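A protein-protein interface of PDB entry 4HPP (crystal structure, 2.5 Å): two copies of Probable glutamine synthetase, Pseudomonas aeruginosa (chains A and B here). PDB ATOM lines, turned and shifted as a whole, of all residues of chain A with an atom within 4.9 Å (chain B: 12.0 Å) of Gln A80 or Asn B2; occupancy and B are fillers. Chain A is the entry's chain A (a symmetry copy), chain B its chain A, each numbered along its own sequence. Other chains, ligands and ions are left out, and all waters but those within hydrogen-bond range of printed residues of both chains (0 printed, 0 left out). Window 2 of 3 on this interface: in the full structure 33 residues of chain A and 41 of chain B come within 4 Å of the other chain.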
ATOM      1  N   VAL A  78      -0.047  23.133  18.732  1.00  0.00           N
ATOM      2  CA  VAL A  78      -0.389  23.472  20.127  1.00  0.00           C
ATOM      3  C   VAL A  78       0.927  23.877  20.746  1.00  0.00           C
ATOM      4  O   VAL A  78       1.809  23.028  20.977  1.00  0.00           O
ATOM      5  CB  VAL A  78      -0.953  22.270  20.942  1.00  0.00           C
ATOM      6  CG1 VAL A  78      -1.245  22.669  22.393  1.00  0.00           C
ATOM      7  CG2 VAL A  78      -2.134  21.549  20.214  1.00  0.00           C
ATOM      8  N   GLU A  79       1.063  25.177  21.015  1.00  0.00           N
ATOM      9  CA  GLU A  79       2.325  25.724  21.473  1.00  0.00           C
ATOM     10  C   GLU A  79       2.484  25.478  22.943  1.00  0.00           C
ATOM     11  O   GLU A  79       3.590  25.239  23.421  1.00  0.00           O
ATOM     12  CB  GLU A  79       2.401  27.216  21.144  1.00  0.00           C
ATOM     13  CG  GLU A  79       2.241  27.460  19.627  1.00  0.00           C
ATOM     14  CD  GLU A  79       3.492  27.060  18.820  1.00  0.00           C
ATOM     15  OE1 GLU A  79       4.574  26.997  19.431  1.00  0.00           O
ATOM     16  OE2 GLU A  79       3.417  26.784  17.584  1.00  0.00           O
ATOM     17  N   GLN A  80       1.389  25.517  23.689  1.00  0.00           N
ATOM     18  CA  GLN A  80       1.553  25.366  25.132  1.00  0.00           C
ATOM     19  C   GLN A  80       0.517  24.496  25.755  1.00  0.00           C
ATOM     20  O   GLN A  80      -0.682  24.649  25.456  1.00  0.00           O
ATOM     21  CB  GLN A  80       1.478  26.703  25.790  1.00  0.00           C
ATOM     22  CG  GLN A  80       2.850  27.274  26.047  1.00  0.00           C
ATOM     23  CD  GLN A  80       2.731  28.718  26.392  1.00  0.00           C
ATOM     24  OE1 GLN A  80       2.368  29.517  25.538  1.00  0.00           O
ATOM     25  NE2 GLN A  80       2.969  29.058  27.658  1.00  0.00           N
ATOM     26  N   GLY A  81       0.960  23.597  26.628  1.00  0.00           N
ATOM     27  CA  GLY A  81       0.011  22.782  27.369  1.00  0.00           C
ATOM     28  C   GLY A  81       0.281  22.916  28.843  1.00  0.00           C
ATOM     29  O   GLY A  81       1.054  23.777  29.251  1.00  0.00           O
ATOM     30  N   PRO A  82      -0.312  22.021  29.643  1.00  0.00           N
ATOM     31  CA  PRO A  82      -0.236  22.061  31.088  1.00  0.00           C
ATOM     32  C   PRO A  82       1.188  22.136  31.656  1.00  0.00           C
ATOM     33  O   PRO A  82       1.427  22.748  32.704  1.00  0.00           O
ATOM     34  CB  PRO A  82      -0.927  20.765  31.511  1.00  0.00           C
ATOM     35  CG  PRO A  82      -1.566  20.197  30.276  1.00  0.00           C
ATOM     36  CD  PRO A  82      -1.389  21.153  29.166  1.00  0.00           C
ATOM     37  N   TRP A 162      -7.340  23.149  30.529  1.00  0.00           N
ATOM     38  CA  TRP A 162      -6.171  22.964  29.638  1.00  0.00           C
ATOM     39  C   TRP A 162      -6.514  22.166  28.438  1.00  0.00           C
ATOM     40  O   TRP A 162      -5.856  22.248  27.412  1.00  0.00           O
ATOM     41  CB  TRP A 162      -5.005  22.304  30.337  1.00  0.00           C
ATOM     42  CG  TRP A 162      -4.090  23.320  30.923  1.00  0.00           C
ATOM     43  CD1 TRP A 162      -3.816  23.522  32.264  1.00  0.00           C
ATOM     44  CD2 TRP A 162      -3.287  24.326  30.210  1.00  0.00           C
ATOM     45  NE1 TRP A 162      -2.917  24.545  32.437  1.00  0.00           N
ATOM     46  CE2 TRP A 162      -2.569  25.082  31.239  1.00  0.00           C
ATOM     47  CE3 TRP A 162      -3.118  24.684  28.869  1.00  0.00           C
ATOM     48  CZ2 TRP A 162      -1.729  26.172  30.917  1.00  0.00           C
ATOM     49  CZ3 TRP A 162      -2.261  25.747  28.561  1.00  0.00           C
ATOM     50  CH2 TRP A 162      -1.590  26.475  29.566  1.00  0.00           C
ATOM     51  N   GLN A 169      -6.158  26.025  20.624  1.00  0.00           N
ATOM     52  CA  GLN A 169      -4.898  26.235  19.919  1.00  0.00           C
ATOM     53  C   GLN A 169      -4.757  25.308  18.756  1.00  0.00           C
ATOM     54  O   GLN A 169      -4.160  25.662  17.798  1.00  0.00           O
ATOM     55  CB  GLN A 169      -3.671  26.000  20.794  1.00  0.00           C
ATOM     56  CG  GLN A 169      -3.493  26.883  22.019  1.00  0.00           C
ATOM     57  CD  GLN A 169      -2.397  26.365  22.866  1.00  0.00           C
ATOM     58  OE1 GLN A 169      -1.278  26.127  22.357  1.00  0.00           O
ATOM     59  NE2 GLN A 169      -2.724  26.017  24.151  1.00  0.00           N
ATOM     60  N   MET B   1       7.021  33.469  25.033  1.00  0.00           N
ATOM     61  CA  MET B   1       6.736  34.934  24.914  1.00  0.00           C
ATOM     62  C   MET B   1       5.751  35.332  26.025  1.00  0.00           C
ATOM     63  O   MET B   1       6.024  36.228  26.830  1.00  0.00           O
ATOM     64  CB  MET B   1       6.177  35.287  23.513  1.00  0.00           C
ATOM     65  CG  MET B   1       6.657  34.401  22.356  1.00  0.00           C
ATOM     66  SD  MET B   1       5.879  32.759  22.260  1.00  0.00           S
ATOM     67  CE  MET B   1       4.365  33.133  21.365  1.00  0.00           C
ATOM     68  N   ASN B   2       4.612  34.635  26.039  1.00  0.00           N
ATOM     69  CA  ASN B   2       3.556  34.761  27.039  1.00  0.00           C
ATOM     70  C   ASN B   2       3.257  33.331  27.523  1.00  0.00           C
ATOM     71  O   ASN B   2       3.196  32.406  26.718  1.00  0.00           O
ATOM     72  CB  ASN B   2       2.309  35.416  26.400  1.00  0.00           C
ATOM     73  CG  ASN B   2       1.244  35.822  27.424  1.00  0.00           C
ATOM     74  OD1 ASN B   2       0.329  35.048  27.759  1.00  0.00           O
ATOM     75  ND2 ASN B   2       1.344  37.061  27.906  1.00  0.00           N
ATOM     76  N   ARG B   3       3.119  33.124  28.829  1.00  0.00           N
ATOM     77  CA  ARG B   3       2.690  31.814  29.319  1.00  0.00           C
ATOM     78  C   ARG B   3       1.165  31.733  29.194  1.00  0.00           C
ATOM     79  O   ARG B   3       0.439  32.483  29.858  1.00  0.00           O
ATOM     80  CB  ARG B   3       3.164  31.568  30.766  1.00  0.00           C
ATOM     81  CG  ARG B   3       2.654  30.271  31.423  1.00  0.00           C
ATOM     82  CD  ARG B   3       3.286  28.996  30.868  1.00  0.00           C
ATOM     83  NE  ARG B   3       2.809  27.780  31.552  1.00  0.00           N
ATOM     84  CZ  ARG B   3       2.231  26.716  30.958  1.00  0.00           C
ATOM     85  NH1 ARG B   3       2.016  26.651  29.621  1.00  0.00           N
ATOM     86  NH2 ARG B   3       1.868  25.683  31.706  1.00  0.00           N
ATOM     87  N   LEU B   4       0.672  30.831  28.341  1.00  0.00           N
ATOM     88  CA  LEU B   4      -0.774  30.737  28.101  1.00  0.00           C
ATOM     89  C   LEU B   4      -1.563  30.308  29.341  1.00  0.00           C
ATOM     90  O   LEU B   4      -1.008  29.715  30.296  1.00  0.00           O
ATOM     91  CB  LEU B   4      -1.097  29.849  26.882  1.00  0.00           C
ATOM     92  CG  LEU B   4      -1.495  30.557  25.574  1.00  0.00           C
ATOM     93  CD1 LEU B   4      -0.830  29.923  24.360  1.00  0.00           C
ATOM     94  CD2 LEU B   4      -3.012  30.636  25.385  1.00  0.00           C
ATOM     95  N   GLN B   5      -2.848  30.648  29.297  1.00  0.00           N
ATOM     96  CA  GLN B   5      -3.849  30.326  30.303  1.00  0.00           C
ATOM     97  C   GLN B   5      -4.770  29.181  29.840  1.00  0.00           C
ATOM     98  O   GLN B   5      -5.103  29.062  28.647  1.00  0.00           O
ATOM     99  CB  GLN B   5      -4.749  31.544  30.545  1.00  0.00           C
ATOM    100  CG  GLN B   5      -4.045  32.863  30.848  1.00  0.00           C
ATOM    101  CD  GLN B   5      -3.294  32.819  32.167  1.00  0.00           C
ATOM    102  OE1 GLN B   5      -2.135  33.205  32.225  1.00  0.00           O
ATOM    103  NE2 GLN B   5      -3.946  32.330  33.230  1.00  0.00           N
ATOM    104  N   PRO B   6      -5.166  28.312  30.790  1.00  0.00           N
ATOM    105  CA  PRO B   6      -6.294  27.373  30.670  1.00  0.00           C
ATOM    106  C   PRO B   6      -7.585  28.111  30.381  1.00  0.00           C
ATOM    107  O   PRO B   6      -7.765  29.251  30.818  1.00  0.00           O
ATOM    108  CB  PRO B   6      -6.372  26.737  32.055  1.00  0.00           C
ATOM    109  CG  PRO B   6      -5.210  27.259  32.839  1.00  0.00           C
ATOM    110  CD  PRO B   6      -4.294  27.977  31.929  1.00  0.00           C
ATOM    111  N   VAL B   7      -8.474  27.525  29.610  1.00  0.00           N
ATOM    112  CA  VAL B   7      -9.702  28.240  29.284  1.00  0.00           C
ATOM    113  C   VAL B   7     -10.592  28.269  30.531  1.00  0.00           C
ATOM    114  O   VAL B   7     -10.595  27.329  31.314  1.00  0.00           O
ATOM    115  CB  VAL B   7     -10.353  27.692  27.947  1.00  0.00           C
ATOM    116  CG1 VAL B   7     -11.812  28.036  27.787  1.00  0.00           C
ATOM    117  CG2 VAL B   7      -9.625  28.246  26.717  1.00  0.00           C
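Of chain B, only Asn B2 (3.2 Å), Arg B3 (3.2 Å) and Leu B4 (3.0 Å) come within 4 Å of Gln A80. Of chain B, only Arg B3 (3.1 Å) comes within 4 Å of Gly A81. Pro A82 touches just one residue of chain B: Arg B3 (3.1 Å). Of the printed residues of chain B, Trp A162 touches Arg B3 (3.6 Å), Leu B4 (3.4 Å) and Pro B6 (3.3 Å). Met B1 touches none of the printed residues of chain A. Asn B2 touches one residue of chain A. Of the printed residues of chain A, Arg B3 touches Gln A80 (3.2 Å), Gly A81 (3.1 Å), Pro A82 (3.1 Å) and Trp A162 (3.6 Å). Of the printed residues of chain A, Leu B4 touches Gln A80 and Trp A162. Gln B5 touches none of the printed residues of chain A. Printed residues of chain A within 4 Å of Pro B6: Trp A162. The nearest residue of chain B that does not touch Gln A80 is Met B1 (5.8 Å). The nearest printed residue of chain A that does not touch Arg B3 is Glu A79 (6.6 Å).
No position is printed for both chains.
O of Gln A80 sits at hydrogen-bond distance from NE2 of Gln A169 (2.8 Å).
Of the 7 printed residues of chain B, 4 touch a printed residue of chain A. Of the 7 printed residues of chain A, 4 touch a printed residue of chain B. Hydrophobic or aromatic side chains of chain A within 4 Å of the printed part of chain B: Trp A162. Among the printed residues, 8 pairs touch across the chains. Among the printed residues, no Asp or Glu carboxylate lies within 4 Å of a Lys or Arg side-chain nitrogen of the other chain.
Trp A162 touches Arg B3. Leu B4 touches Trp A162. Trp A162 touches Pro B6.
The backbone carbonyl oxygen (O) of Asn B2 sits close to the side-chain amide oxygen (OE1) of Gln A80 (3.2 Å). The side-chain amide nitrogen (NE2) of Gln A80 lies close to the guanidinium group (NH1) of Arg B3 (3.2 Å). The backbone carbonyl oxygen of Gly A81 sits at hydrogen-bond distance from the guanidinium group of Arg B3 (3.1 Å). The backbone carbonyl oxygen (O) of Pro A82 sits at hydrogen-bond distance from the guanidinium group (NH2) of Arg B3 (3.1 Å). The side-chain amide nitrogen (NE2) of Gln A80 sits close to the backbone NH (N) of Leu B4.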
